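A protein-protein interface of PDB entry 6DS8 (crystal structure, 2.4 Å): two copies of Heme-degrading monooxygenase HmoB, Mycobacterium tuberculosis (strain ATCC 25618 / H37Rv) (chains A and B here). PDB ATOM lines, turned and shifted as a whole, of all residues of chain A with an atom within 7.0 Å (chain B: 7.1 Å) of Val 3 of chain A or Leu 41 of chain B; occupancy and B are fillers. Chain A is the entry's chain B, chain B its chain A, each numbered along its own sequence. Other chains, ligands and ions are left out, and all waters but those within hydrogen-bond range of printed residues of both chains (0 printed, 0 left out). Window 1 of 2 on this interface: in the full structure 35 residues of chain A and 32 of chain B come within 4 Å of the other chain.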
ATOM      1  N   PRO A   1      -2.304 -15.182 -20.438  1.00  0.00           N
ATOM      2  CA  PRO A   1      -2.985 -16.436 -20.130  1.00  0.00           C
ATOM      3  C   PRO A   1      -3.227 -17.301 -21.349  1.00  0.00           C
ATOM      4  O   PRO A   1      -3.222 -16.748 -22.454  1.00  0.00           O
ATOM      5  CB  PRO A   1      -4.323 -15.944 -19.552  1.00  0.00           C
ATOM      6  CG  PRO A   1      -3.912 -14.707 -18.769  1.00  0.00           C
ATOM      7  CD  PRO A   1      -2.710 -14.115 -19.496  1.00  0.00           C
ATOM      8  N   VAL A   2      -3.509 -18.601 -21.154  1.00  0.00           N
ATOM      9  CA  VAL A   2      -3.809 -19.498 -22.258  1.00  0.00           C
ATOM     10  C   VAL A   2      -5.151 -20.148 -21.989  1.00  0.00           C
ATOM     11  O   VAL A   2      -5.649 -20.182 -20.860  1.00  0.00           O
ATOM     12  CB  VAL A   2      -2.714 -20.574 -22.509  1.00  0.00           C
ATOM     13  CG1 VAL A   2      -1.435 -19.914 -23.084  1.00  0.00           C
ATOM     14  CG2 VAL A   2      -2.392 -21.395 -21.241  1.00  0.00           C
ATOM     15  N   VAL A   3      -5.749 -20.655 -23.054  1.00  0.00           N
ATOM     16  CA  VAL A   3      -6.964 -21.433 -22.943  1.00  0.00           C
ATOM     17  C   VAL A   3      -6.778 -22.725 -23.721  1.00  0.00           C
ATOM     18  O   VAL A   3      -6.373 -22.708 -24.899  1.00  0.00           O
ATOM     19  CB  VAL A   3      -8.194 -20.653 -23.436  1.00  0.00           C
ATOM     20  CG1 VAL A   3      -9.371 -21.625 -23.732  1.00  0.00           C
ATOM     21  CG2 VAL A   3      -8.559 -19.602 -22.392  1.00  0.00           C
ATOM     22  N   LYS A   4      -7.082 -23.848 -23.051  1.00  0.00           N
ATOM     23  CA  LYS A   4      -7.065 -25.171 -23.659  1.00  0.00           C
ATOM     24  C   LYS A   4      -8.473 -25.727 -23.602  1.00  0.00           C
ATOM     25  O   LYS A   4      -8.954 -26.099 -22.532  1.00  0.00           O
ATOM     26  CB  LYS A   4      -6.085 -26.096 -22.937  1.00  0.00           C
ATOM     27  CG  LYS A   4      -4.736 -25.433 -22.607  1.00  0.00           C
ATOM     28  CD  LYS A   4      -3.868 -25.180 -23.841  1.00  0.00           C
ATOM     29  CE  LYS A   4      -2.448 -24.703 -23.434  1.00  0.00           C
ATOM     30  NZ  LYS A   4      -1.570 -24.530 -24.615  1.00  0.00           N
ATOM     31  N   ILE A   5      -9.135 -25.795 -24.744  1.00  0.00           N
ATOM     32  CA  ILE A   5     -10.435 -26.435 -24.817  1.00  0.00           C
ATOM     33  C   ILE A   5     -10.250 -27.862 -25.300  1.00  0.00           C
ATOM     34  O   ILE A   5      -9.830 -28.086 -26.443  1.00  0.00           O
ATOM     35  CB  ILE A   5     -11.390 -25.698 -25.761  1.00  0.00           C
ATOM     36  CG1 ILE A   5     -11.398 -24.191 -25.506  1.00  0.00           C
ATOM     37  CG2 ILE A   5     -12.771 -26.320 -25.625  1.00  0.00           C
ATOM     38  CD1 ILE A   5     -12.284 -23.485 -26.494  1.00  0.00           C
ATOM     39  N   VAL A  52     -14.728 -28.636 -22.983  1.00  0.00           N
ATOM     40  CA  VAL A  52     -14.126 -28.508 -21.665  1.00  0.00           C
ATOM     41  C   VAL A  52     -13.144 -27.355 -21.762  1.00  0.00           C
ATOM     42  O   VAL A  52     -12.025 -27.521 -22.273  1.00  0.00           O
ATOM     43  CB  VAL A  52     -13.429 -29.797 -21.211  1.00  0.00           C
ATOM     44  CG1 VAL A  52     -12.874 -29.607 -19.783  1.00  0.00           C
ATOM     45  CG2 VAL A  52     -14.361 -31.020 -21.343  1.00  0.00           C
ATOM     46  N   VAL A  53     -13.540 -26.196 -21.249  1.00  0.00           N
ATOM     47  CA  VAL A  53     -12.764 -24.969 -21.398  1.00  0.00           C
ATOM     48  C   VAL A  53     -11.894 -24.754 -20.156  1.00  0.00           C
ATOM     49  O   VAL A  53     -12.413 -24.503 -19.064  1.00  0.00           O
ATOM     50  CB  VAL A  53     -13.701 -23.783 -21.649  1.00  0.00           C
ATOM     51  CG1 VAL A  53     -12.919 -22.525 -21.930  1.00  0.00           C
ATOM     52  CG2 VAL A  53     -14.609 -24.129 -22.833  1.00  0.00           C
ATOM     53  N   THR A  54     -10.564 -24.821 -20.306  1.00  0.00           N
ATOM     54  CA  THR A  54      -9.660 -24.710 -19.154  1.00  0.00           C
ATOM     55  C   THR A  54      -8.772 -23.481 -19.297  1.00  0.00           C
ATOM     56  O   THR A  54      -8.401 -23.088 -20.408  1.00  0.00           O
ATOM     57  CB  THR A  54      -8.825 -25.986 -18.972  1.00  0.00           C
ATOM     58  OG1 THR A  54      -7.783 -26.052 -19.961  1.00  0.00           O
ATOM     59  CG2 THR A  54      -9.736 -27.258 -19.054  1.00  0.00           C
ATOM     60  N   HIS A  55      -8.508 -22.807 -18.188  1.00  0.00           N
ATOM     61  CA  HIS A  55      -7.788 -21.542 -18.231  1.00  0.00           C
ATOM     62  C   HIS A  55      -6.487 -21.683 -17.457  1.00  0.00           C
ATOM     63  O   HIS A  55      -6.482 -22.234 -16.344  1.00  0.00           O
ATOM     64  CB  HIS A  55      -8.608 -20.408 -17.630  1.00  0.00           C
ATOM     65  CG  HIS A  55      -9.909 -20.142 -18.321  1.00  0.00           C
ATOM     66  ND1 HIS A  55     -10.075 -19.109 -19.225  1.00  0.00           N
ATOM     67  CD2 HIS A  55     -11.132 -20.718 -18.184  1.00  0.00           C
ATOM     68  CE1 HIS A  55     -11.334 -19.076 -19.637  1.00  0.00           C
ATOM     69  NE2 HIS A  55     -11.995 -20.048 -19.030  1.00  0.00           N
ATOM     70  N   TRP A  56      -5.384 -21.170 -18.019  1.00  0.00           N
ATOM     71  CA  TRP A  56      -4.088 -21.340 -17.363  1.00  0.00           C
ATOM     72  C   TRP A  56      -3.242 -20.083 -17.479  1.00  0.00           C
ATOM     73  O   TRP A  56      -3.341 -19.341 -18.457  1.00  0.00           O
ATOM     74  CB  TRP A  56      -3.300 -22.521 -17.946  1.00  0.00           C
ATOM     75  CG  TRP A  56      -4.053 -23.791 -17.948  1.00  0.00           C
ATOM     76  CD1 TRP A  56      -4.933 -24.212 -18.893  1.00  0.00           C
ATOM     77  CD2 TRP A  56      -4.003 -24.820 -16.948  1.00  0.00           C
ATOM     78  NE1 TRP A  56      -5.433 -25.439 -18.561  1.00  0.00           N
ATOM     79  CE2 TRP A  56      -4.875 -25.845 -17.372  1.00  0.00           C
ATOM     80  CE3 TRP A  56      -3.293 -24.981 -15.748  1.00  0.00           C
ATOM     81  CZ2 TRP A  56      -5.078 -27.015 -16.625  1.00  0.00           C
ATOM     82  CZ3 TRP A  56      -3.497 -26.141 -15.004  1.00  0.00           C
ATOM     83  CH2 TRP A  56      -4.387 -27.140 -15.444  1.00  0.00           C
ATOM     84  N   LEU A  88      -7.788 -31.431 -28.938  1.00  0.00           N
ATOM     85  CA  LEU A  88      -7.330 -30.325 -28.113  1.00  0.00           C
ATOM     86  C   LEU A  88      -7.228 -29.039 -28.927  1.00  0.00           C
ATOM     87  O   LEU A  88      -6.442 -28.966 -29.883  1.00  0.00           O
ATOM     88  CB  LEU A  88      -5.982 -30.704 -27.512  1.00  0.00           C
ATOM     89  CG  LEU A  88      -5.386 -29.715 -26.544  1.00  0.00           C
ATOM     90  CD1 LEU A  88      -6.353 -29.487 -25.361  1.00  0.00           C
ATOM     91  CD2 LEU A  88      -4.007 -30.261 -26.119  1.00  0.00           C
ATOM     92  N   LEU A  89      -7.987 -28.011 -28.537  1.00  0.00           N
ATOM     93  CA  LEU A  89      -7.921 -26.695 -29.179  1.00  0.00           C
ATOM     94  C   LEU A  89      -7.219 -25.741 -28.219  1.00  0.00           C
ATOM     95  O   LEU A  89      -7.631 -25.608 -27.057  1.00  0.00           O
ATOM     96  CB  LEU A  89      -9.307 -26.161 -29.557  1.00  0.00           C
ATOM     97  CG  LEU A  89     -10.357 -27.169 -30.061  1.00  0.00           C
ATOM     98  CD1 LEU A  89     -11.708 -26.469 -30.369  1.00  0.00           C
ATOM     99  CD2 LEU A  89      -9.882 -27.987 -31.266  1.00  0.00           C
ATOM    100  N   GLU A  90      -6.147 -25.102 -28.687  1.00  0.00           N
ATOM    101  CA  GLU A  90      -5.240 -24.357 -27.822  1.00  0.00           C
ATOM    102  C   GLU A  90      -5.188 -22.920 -28.268  1.00  0.00           C
ATOM    103  O   GLU A  90      -5.022 -22.651 -29.450  1.00  0.00           O
ATOM    104  CB  GLU A  90      -3.860 -24.980 -27.850  1.00  0.00           C
ATOM    105  CG  GLU A  90      -3.959 -26.476 -27.785  1.00  0.00           C
ATOM    106  CD  GLU A  90      -2.646 -27.147 -27.495  1.00  0.00           C
ATOM    107  OE1 GLU A  90      -1.928 -26.687 -26.588  1.00  0.00           O
ATOM    108  OE2 GLU A  90      -2.357 -28.139 -28.182  1.00  0.00           O
ATOM    109  N   PHE A  91      -5.314 -21.999 -27.330  1.00  0.00           N
ATOM    110  CA  PHE A  91      -5.454 -20.600 -27.693  1.00  0.00           C
ATOM    111  C   PHE A  91      -4.575 -19.735 -26.801  1.00  0.00           C
ATOM    112  O   PHE A  91      -4.172 -20.127 -25.705  1.00  0.00           O
ATOM    113  CB  PHE A  91      -6.928 -20.109 -27.579  1.00  0.00           C
ATOM    114  CG  PHE A  91      -7.912 -20.831 -28.498  1.00  0.00           C
ATOM    115  CD1 PHE A  91      -8.525 -22.014 -28.096  1.00  0.00           C
ATOM    116  CD2 PHE A  91      -8.249 -20.293 -29.753  1.00  0.00           C
ATOM    117  CE1 PHE A  91      -9.473 -22.652 -28.939  1.00  0.00           C
ATOM    118  CE2 PHE A  91      -9.162 -20.903 -30.591  1.00  0.00           C
ATOM    119  CZ  PHE A  91      -9.780 -22.091 -30.192  1.00  0.00           C
ATOM    120  N   GLU A  92      -4.290 -18.536 -27.286  1.00  0.00           N
ATOM    121  CA  GLU A  92      -3.725 -17.475 -26.474  1.00  0.00           C
ATOM    122  C   GLU A  92      -4.814 -16.443 -26.201  1.00  0.00           C
ATOM    123  O   GLU A  92      -5.636 -16.155 -27.080  1.00  0.00           O
ATOM    124  CB  GLU A  92      -2.519 -16.850 -27.186  1.00  0.00           C
ATOM    125  CG  GLU A  92      -1.863 -15.695 -26.475  1.00  0.00           C
ATOM    126  CD  GLU A  92      -0.874 -16.155 -25.414  1.00  0.00           C
ATOM    127  OE1 GLU A  92      -0.292 -17.271 -25.584  1.00  0.00           O
ATOM    128  OE2 GLU A  92      -0.698 -15.401 -24.419  1.00  0.00           O
ATOM    129  N   VAL A  93      -4.896 -15.967 -24.959  1.00  0.00           N
ATOM    130  CA  VAL A  93      -5.849 -14.912 -24.609  1.00  0.00           C
ATOM    131  C   VAL A  93      -5.304 -13.575 -25.120  1.00  0.00           C
ATOM    132  O   VAL A  93      -4.284 -13.080 -24.640  1.00  0.00           O
ATOM    133  CB  VAL A  93      -6.134 -14.852 -23.099  1.00  0.00           C
ATOM    134  CG1 VAL A  93      -7.136 -13.734 -22.816  1.00  0.00           C
ATOM    135  CG2 VAL A  93      -6.664 -16.236 -22.560  1.00  0.00           C
ATOM    136  N   VAL A  94      -5.963 -13.004 -26.118  1.00  0.00           N
ATOM    137  CA  VAL A  94      -5.530 -11.715 -26.628  1.00  0.00           C
ATOM    138  C   VAL A  94      -6.274 -10.568 -25.944  1.00  0.00           C
ATOM    139  O   VAL A  94      -5.720  -9.471 -25.774  1.00  0.00           O
ATOM    140  CB  VAL A  94      -5.697 -11.709 -28.162  1.00  0.00           C
ATOM    141  CG1 VAL A  94      -5.898 -10.351 -28.705  1.00  0.00           C
ATOM    142  CG2 VAL A  94      -4.477 -12.302 -28.784  1.00  0.00           C
ATOM    143  N   LEU A  95      -7.515 -10.804 -25.521  1.00  0.00           N
ATOM    144  CA  LEU A  95      -8.320  -9.746 -24.934  1.00  0.00           C
ATOM    145  C   LEU A  95      -9.294 -10.341 -23.922  1.00  0.00           C
ATOM    146  O   LEU A  95      -9.957 -11.337 -24.213  1.00  0.00           O
ATOM    147  CB  LEU A  95      -9.055  -8.995 -26.042  1.00  0.00           C
ATOM    148  CG  LEU A  95      -9.966  -7.914 -25.535  1.00  0.00           C
ATOM    149  CD1 LEU A  95      -9.061  -6.750 -25.186  1.00  0.00           C
ATOM    150  CD2 LEU A  95     -10.978  -7.581 -26.650  1.00  0.00           C
ATOM    151  N   ILE B   5     -19.816 -18.750 -28.367  1.00  0.00           N
ATOM    152  CA  ILE B   5     -18.528 -18.550 -29.026  1.00  0.00           C
ATOM    153  C   ILE B   5     -18.792 -18.240 -30.487  1.00  0.00           C
ATOM    154  O   ILE B   5     -19.380 -19.062 -31.196  1.00  0.00           O
ATOM    155  CB  ILE B   5     -17.634 -19.797 -28.902  1.00  0.00           C
ATOM    156  CG1 ILE B   5     -17.545 -20.244 -27.435  1.00  0.00           C
ATOM    157  CG2 ILE B   5     -16.264 -19.539 -29.525  1.00  0.00           C
ATOM    158  CD1 ILE B   5     -16.703 -21.493 -27.229  1.00  0.00           C
ATOM    159  N   ILE B   8     -14.551 -17.434 -35.798  1.00  0.00           N
ATOM    160  CA  ILE B   8     -14.323 -16.633 -37.022  1.00  0.00           C
ATOM    161  C   ILE B   8     -13.075 -17.061 -37.785  1.00  0.00           C
ATOM    162  O   ILE B   8     -12.016 -17.206 -37.218  1.00  0.00           O
ATOM    163  CB  ILE B   8     -14.385 -15.128 -36.728  1.00  0.00           C
ATOM    164  CG1 ILE B   8     -13.233 -14.669 -35.845  1.00  0.00           C
ATOM    165  CG2 ILE B   8     -15.714 -14.786 -36.109  1.00  0.00           C
ATOM    166  CD1 ILE B   8     -13.347 -13.232 -35.410  1.00  0.00           C
ATOM    167  N   LEU B  18      -7.256  -8.259 -37.427  1.00  0.00           N
ATOM    168  CA  LEU B  18      -8.488  -8.650 -36.753  1.00  0.00           C
ATOM    169  C   LEU B  18      -8.445  -8.286 -35.271  1.00  0.00           C
ATOM    170  O   LEU B  18      -9.399  -7.717 -34.727  1.00  0.00           O
ATOM    171  CB  LEU B  18      -8.727 -10.146 -36.931  1.00  0.00           C
ATOM    172  CG  LEU B  18      -9.925 -10.587 -36.074  1.00  0.00           C
ATOM    173  CD1 LEU B  18     -11.169 -10.521 -36.876  1.00  0.00           C
ATOM    174  CD2 LEU B  18      -9.770 -11.915 -35.453  1.00  0.00           C
ATOM    175  N   GLU B  19      -7.326  -8.573 -34.613  1.00  0.00           N
ATOM    176  CA  GLU B  19      -7.181  -8.265 -33.193  1.00  0.00           C
ATOM    177  C   GLU B  19      -7.206  -6.776 -32.936  1.00  0.00           C
ATOM    178  O   GLU B  19      -7.657  -6.343 -31.877  1.00  0.00           O
ATOM    179  CB  GLU B  19      -5.865  -8.861 -32.648  1.00  0.00           C
ATOM    180  CG  GLU B  19      -5.851 -10.381 -32.669  1.00  0.00           C
ATOM    181  CD  GLU B  19      -4.490 -10.965 -32.333  1.00  0.00           C
ATOM    182  OE1 GLU B  19      -4.254 -12.124 -32.737  1.00  0.00           O
ATOM    183  OE2 GLU B  19      -3.664 -10.269 -31.671  1.00  0.00           O
ATOM    184  N   PHE B  38     -16.159 -11.576 -21.734  1.00  0.00           N
ATOM    185  CA  PHE B  38     -15.806 -12.210 -22.991  1.00  0.00           C
ATOM    186  C   PHE B  38     -14.308 -12.148 -23.203  1.00  0.00           C
ATOM    187  O   PHE B  38     -13.631 -11.264 -22.680  1.00  0.00           O
ATOM    188  CB  PHE B  38     -16.565 -11.573 -24.174  1.00  0.00           C
ATOM    189  CG  PHE B  38     -15.811 -10.520 -24.936  1.00  0.00           C
ATOM    190  CD1 PHE B  38     -15.900  -9.186 -24.573  1.00  0.00           C
ATOM    191  CD2 PHE B  38     -15.106 -10.843 -26.096  1.00  0.00           C
ATOM    192  CE1 PHE B  38     -15.257  -8.207 -25.309  1.00  0.00           C
ATOM    193  CE2 PHE B  38     -14.458  -9.858 -26.843  1.00  0.00           C
ATOM    194  CZ  PHE B  38     -14.538  -8.548 -26.443  1.00  0.00           C
ATOM    195  N   GLN B  39     -13.799 -13.105 -23.972  1.00  0.00           N
ATOM    196  CA  GLN B  39     -12.386 -13.134 -24.323  1.00  0.00           C
ATOM    197  C   GLN B  39     -12.253 -13.233 -25.834  1.00  0.00           C
ATOM    198  O   GLN B  39     -13.028 -13.945 -26.478  1.00  0.00           O
ATOM    199  CB  GLN B  39     -11.615 -14.321 -23.681  1.00  0.00           C
ATOM    200  CG  GLN B  39     -11.923 -14.635 -22.221  1.00  0.00           C
ATOM    201  CD  GLN B  39     -11.122 -15.871 -21.697  1.00  0.00           C
ATOM    202  OE1 GLN B  39     -11.414 -17.044 -22.036  1.00  0.00           O
ATOM    203  NE2 GLN B  39     -10.107 -15.600 -20.872  1.00  0.00           N
ATOM    204  N   LEU B  40     -11.258 -12.539 -26.402  1.00  0.00           N
ATOM    205  CA  LEU B  40     -10.841 -12.844 -27.763  1.00  0.00           C
ATOM    206  C   LEU B  40      -9.712 -13.867 -27.663  1.00  0.00           C
ATOM    207  O   LEU B  40      -8.750 -13.676 -26.911  1.00  0.00           O
ATOM    208  CB  LEU B  40     -10.403 -11.596 -28.534  1.00  0.00           C
ATOM    209  CG  LEU B  40      -9.906 -11.853 -29.973  1.00  0.00           C
ATOM    210  CD1 LEU B  40     -11.014 -12.526 -30.828  1.00  0.00           C
ATOM    211  CD2 LEU B  40      -9.352 -10.598 -30.702  1.00  0.00           C
ATOM    212  N   LEU B  41      -9.868 -14.975 -28.379  1.00  0.00           N
ATOM    213  CA  LEU B  41      -8.922 -16.073 -28.269  1.00  0.00           C
ATOM    214  C   LEU B  41      -8.300 -16.324 -29.627  1.00  0.00           C
ATOM    215  O   LEU B  41      -8.996 -16.728 -30.573  1.00  0.00           O
ATOM    216  CB  LEU B  41      -9.606 -17.341 -27.752  1.00  0.00           C
ATOM    217  CG  LEU B  41     -10.106 -17.377 -26.306  1.00  0.00           C
ATOM    218  CD1 LEU B  41     -10.437 -18.804 -25.948  1.00  0.00           C
ATOM    219  CD2 LEU B  41      -9.037 -16.887 -25.367  1.00  0.00           C
ATOM    220  N   ARG B  42      -6.928 -16.156 -29.642  1.00  0.00           N
ATOM    221  CA  ARG B  42      -6.086 -16.345 -30.812  1.00  0.00           C
ATOM    222  C   ARG B  42      -5.706 -17.812 -30.925  1.00  0.00           C
ATOM    223  O   ARG B  42      -5.252 -18.404 -29.943  1.00  0.00           O
ATOM    224  CB  ARG B  42      -4.838 -15.483 -30.723  1.00  0.00           C
ATOM    225  CG  ARG B  42      -3.910 -15.600 -31.936  1.00  0.00           C
ATOM    226  CD  ARG B  42      -2.516 -15.157 -31.559  1.00  0.00           C
ATOM    227  NE  ARG B  42      -2.498 -13.722 -31.276  1.00  0.00           N
ATOM    228  CZ  ARG B  42      -1.677 -13.134 -30.420  1.00  0.00           C
ATOM    229  NH1 ARG B  42      -0.823 -13.856 -29.731  1.00  0.00           N
ATOM    230  NH2 ARG B  42      -1.693 -11.817 -30.278  1.00  0.00           N
ATOM    231  N   PRO B  43      -5.907 -18.444 -32.071  1.00  0.00           N
ATOM    232  CA  PRO B  43      -5.613 -19.870 -32.164  1.00  0.00           C
ATOM    233  C   PRO B  43      -4.125 -20.089 -32.234  1.00  0.00           C
ATOM    234  O   PRO B  43      -3.399 -19.306 -32.839  1.00  0.00           O
ATOM    235  CB  PRO B  43      -6.303 -20.286 -33.466  1.00  0.00           C
ATOM    236  CG  PRO B  43      -6.254 -19.050 -34.313  1.00  0.00           C
ATOM    237  CD  PRO B  43      -6.245 -17.860 -33.387  1.00  0.00           C
ATOM    238  N   VAL B  44      -3.690 -21.208 -31.667  1.00  0.00           N
ATOM    239  CA  VAL B  44      -2.280 -21.523 -31.499  1.00  0.00           C
ATOM    240  C   VAL B  44      -2.079 -22.928 -32.022  1.00  0.00           C
ATOM    241  O   VAL B  44      -1.094 -23.210 -32.714  1.00  0.00           O
ATOM    242  CB  VAL B  44      -1.848 -21.397 -30.026  1.00  0.00           C
ATOM    243  CG1 VAL B  44      -0.549 -22.159 -29.771  1.00  0.00           C
ATOM    244  CG2 VAL B  44      -1.664 -19.945 -29.642  1.00  0.00           C
ATOM    245  N   LYS B  45      -3.024 -23.814 -31.728  1.00  0.00           N
ATOM    246  CA  LYS B  45      -2.900 -25.192 -32.174  1.00  0.00           C
ATOM    247  C   LYS B  45      -4.237 -25.909 -32.037  1.00  0.00           C
ATOM    248  O   LYS B  45      -4.951 -25.725 -31.039  1.00  0.00           O
ATOM    249  CB  LYS B  45      -1.815 -25.923 -31.356  1.00  0.00           C
ATOM    250  CG  LYS B  45      -1.465 -27.355 -31.802  1.00  0.00           C
ATOM    251  CD  LYS B  45      -0.274 -27.852 -30.946  1.00  0.00           C
ATOM    252  CE  LYS B  45       0.030 -29.350 -31.155  1.00  0.00           C
ATOM    253  NZ  LYS B  45       1.301 -29.805 -30.475  1.00  0.00           N
ATOM    254  N   ARG B  49      -9.471 -21.050 -36.283  1.00  0.00           N
ATOM    255  CA  ARG B  49     -10.322 -19.877 -36.116  1.00  0.00           C
ATOM    256  C   ARG B  49      -9.993 -19.138 -34.832  1.00  0.00           C
ATOM    257  O   ARG B  49      -9.444 -19.713 -33.880  1.00  0.00           O
ATOM    258  CB  ARG B  49     -11.808 -20.254 -36.115  1.00  0.00           C
ATOM    259  CG  ARG B  49     -12.307 -20.694 -37.471  1.00  0.00           C
ATOM    260  CD  ARG B  49     -13.624 -21.395 -37.351  1.00  0.00           C
ATOM    261  NE  ARG B  49     -13.493 -22.602 -36.571  1.00  0.00           N
ATOM    262  CZ  ARG B  49     -14.513 -23.360 -36.198  1.00  0.00           C
ATOM    263  NH1 ARG B  49     -15.767 -23.024 -36.556  1.00  0.00           N
ATOM    264  NH2 ARG B  49     -14.265 -24.445 -35.451  1.00  0.00           N
ATOM    265  N   TYR B  50     -10.293 -17.834 -34.837  1.00  0.00           N
ATOM    266  CA  TYR B  50     -10.410 -17.088 -33.599  1.00  0.00           C
ATOM    267  C   TYR B  50     -11.722 -17.466 -32.923  1.00  0.00           C
ATOM    268  O   TYR B  50     -12.758 -17.584 -33.579  1.00  0.00           O
ATOM    269  CB  TYR B  50     -10.365 -15.581 -33.878  1.00  0.00           C
ATOM    270  CG  TYR B  50      -8.962 -15.053 -34.043  1.00  0.00           C
ATOM    271  CD1 TYR B  50      -8.237 -15.322 -35.201  1.00  0.00           C
ATOM    272  CD2 TYR B  50      -8.346 -14.304 -33.035  1.00  0.00           C
ATOM    273  CE1 TYR B  50      -6.942 -14.859 -35.368  1.00  0.00           C
ATOM    274  CE2 TYR B  50      -7.060 -13.828 -33.191  1.00  0.00           C
ATOM    275  CZ  TYR B  50      -6.365 -14.114 -34.379  1.00  0.00           C
ATOM    276  OH  TYR B  50      -5.092 -13.668 -34.579  1.00  0.00           O
ATOM    277  N   PHE B  51     -11.675 -17.682 -31.617  1.00  0.00           N
ATOM    278  CA  PHE B  51     -12.865 -17.943 -30.816  1.00  0.00           C
ATOM    279  C   PHE B  51     -13.180 -16.669 -30.033  1.00  0.00           C
ATOM    280  O   PHE B  51     -12.371 -16.247 -29.197  1.00  0.00           O
ATOM    281  CB  PHE B  51     -12.624 -19.105 -29.850  1.00  0.00           C
ATOM    282  CG  PHE B  51     -12.871 -20.497 -30.431  1.00  0.00           C
ATOM    283  CD1 PHE B  51     -12.773 -20.744 -31.793  1.00  0.00           C
ATOM    284  CD2 PHE B  51     -13.190 -21.579 -29.573  1.00  0.00           C
ATOM    285  CE1 PHE B  51     -12.990 -22.045 -32.301  1.00  0.00           C
ATOM    286  CE2 PHE B  51     -13.407 -22.865 -30.079  1.00  0.00           C
ATOM    287  CZ  PHE B  51     -13.302 -23.095 -31.455  1.00  0.00           C
ATOM    288  N   VAL B  52     -14.324 -16.044 -30.309  1.00  0.00           N
ATOM    289  CA  VAL B  52     -14.825 -14.933 -29.493  1.00  0.00           C
ATOM    290  C   VAL B  52     -15.789 -15.538 -28.469  1.00  0.00           C
ATOM    291  O   VAL B  52     -16.933 -15.903 -28.796  1.00  0.00           O
ATOM    292  CB  VAL B  52     -15.494 -13.855 -30.346  1.00  0.00           C
ATOM    293  CG1 VAL B  52     -15.938 -12.679 -29.469  1.00  0.00           C
ATOM    294  CG2 VAL B  52     -14.551 -13.397 -31.471  1.00  0.00           C
ATOM    295  N   VAL B  53     -15.303 -15.703 -27.236  1.00  0.00           N
ATOM    296  CA  VAL B  53     -16.008 -16.435 -26.189  1.00  0.00           C
ATOM    297  C   VAL B  53     -16.725 -15.458 -25.272  1.00  0.00           C
ATOM    298  O   VAL B  53     -16.074 -14.672 -24.566  1.00  0.00           O
ATOM    299  CB  VAL B  53     -15.034 -17.298 -25.387  1.00  0.00           C
ATOM    300  CG1 VAL B  53     -15.799 -18.241 -24.478  1.00  0.00           C
ATOM    301  CG2 VAL B  53     -14.148 -18.055 -26.360  1.00  0.00           C
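Val 53 of chain A touches none of the printed residues of chain B.
Of the printed residues of chain B, His 55 of chain A touches Gln 39 (3.1 Å).
Of the printed residues of chain A, Leu 40 of chain B touches Glu 92 (3.98 Å), Val 93 (3.9 Å), Val 94 (3.0 Å) and Leu 95 (2.8 Å).
Leu 41 of chain B touches just these residues of chain A: Val 3, Phe 91, Glu 92 and Val 93.
Of the printed residues of chain A, Val 44 of chain B touches Glu 90 (3.0 Å) and Glu 92 (3.8 Å).
Printed residues of chain A within 4 Å of Phe 51 of chain B: Ile 5, Leu 89 and Phe 91.
The nearest residue of chain B that does not touch Val 3 of chain A is Val 53 of chain B (6.5 Å).
The nearest printed residue of chain A that does not touch Val 44 of chain B is Phe 91 of chain A (4.1 Å).
Of the 18 printed residues of chain A, 11 touch a printed residue of chain B.
Printed residues of chain A that touch a printed residue of chain B: Val 3, Ile 5, His 55, Leu 88, Leu 89, Glu 90, Phe 91, Glu 92, Val 93, Val 94 and Leu 95.
Among the printed residues, 28 pairs touch across the chains.
Among the printed residues, no Asp or Glu carboxylate lies within 4 Å of a Lys or Arg side-chain nitrogen of the other chain.
The side-chain carboxylate of Glu 19 of chain B is in hydrogen-bond range of the side-chain hydroxyl of Tyr 50 of chain B (2.5 Å).
OE1 of Glu 90 of chain A is in salt-bridge range of NZ of Lys 4 of chain A (2.9 Å).
N of Phe 91 of chain A lies within hydrogen-bond range of O of Val 3 of chain A, at 2.7 Å.
The backbone NH (N) of Val 93 of chain A lies within hydrogen-bond range of the backbone carbonyl oxygen (O) of Pro 1 of chain A, 3.1 Å away.
The backbone NH (N) of Leu 40 of chain B is in hydrogen-bond range of the backbone carbonyl oxygen (O) of Leu 95 of chain A.
N of Glu 92 of chain A lies within hydrogen-bond range of O of Arg 42 of chain B (2.8 Å).
O of Leu 40 of chain B lies within hydrogen-bond range of N of Val 94 of chain A, at 3.0 Å.
The backbone NH (N) of Val 44 of chain B is in hydrogen-bond range of the backbone carbonyl oxygen (O) of Glu 90 of chain A, at 3.0 Å.
O of Lys 45 of chain B lies within hydrogen-bond range of N of Glu 90 of chain A, at 2.7 Å.
Among the printed residues, pairs that only touch across the chains: Leu 95 of chain A with Gln 39 of chain B (3.0 Å), His 55 of chain A with Gln 39 of chain B (3.1 Å), Phe 91 of chain A with Arg 42 of chain B (3.2 Å), Val 94 of chain A with Arg 42 of chain B (3.2 Å), Phe 91 of chain A with Phe 51 of chain B (3.5 Å), Glu 92 of chain A with Leu 41 of chain B (3.5 Å), Phe 91 of chain A with Arg 49 of chain B (3.5 Å), Phe 91 of chain A with Pro 43 of chain B (3.6 Å), Leu 89 of chain A with Lys 45 of chain B (3.6 Å), Val 94 of chain A with Glu 19 of chain B (3.6 Å), Leu 95 of chain A with Phe 38 of chain B (3.7 Å), Ile 5 of chain A with Phe 51 of chain B (3.7 Å), Val 93 of chain A with Leu 41 of chain B (3.7 Å), Phe 91 of chain A with Leu 41 of chain B (3.7 Å), Val 3 of chain A with Leu 41 of chain B (3.7 Å), Leu 88 of chain A with Lys 45 of chain B (3.8 Å), Glu 92 of chain A with Val 44 of chain B (3.8 Å), Val 3 of chain A with Gln 39 of chain B (3.8 Å), Val 93 of chain A with Leu 40 of chain B (3.9 Å), Leu 89 of chain A with Phe 51 of chain B (3.9 Å), Val 93 of chain A with Gln 39 of chain B (3.9 Å), Glu 90 of chain A with Pro 43 of chain B (3.9 Å) and Glu 92 of chain A with Leu 40 of chain B (3.98 Å).
3 positions are printed for both chains.
Of the 28 pairs that touch across the chains among the printed residues, none has its exchanged pair printed and touching as well.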
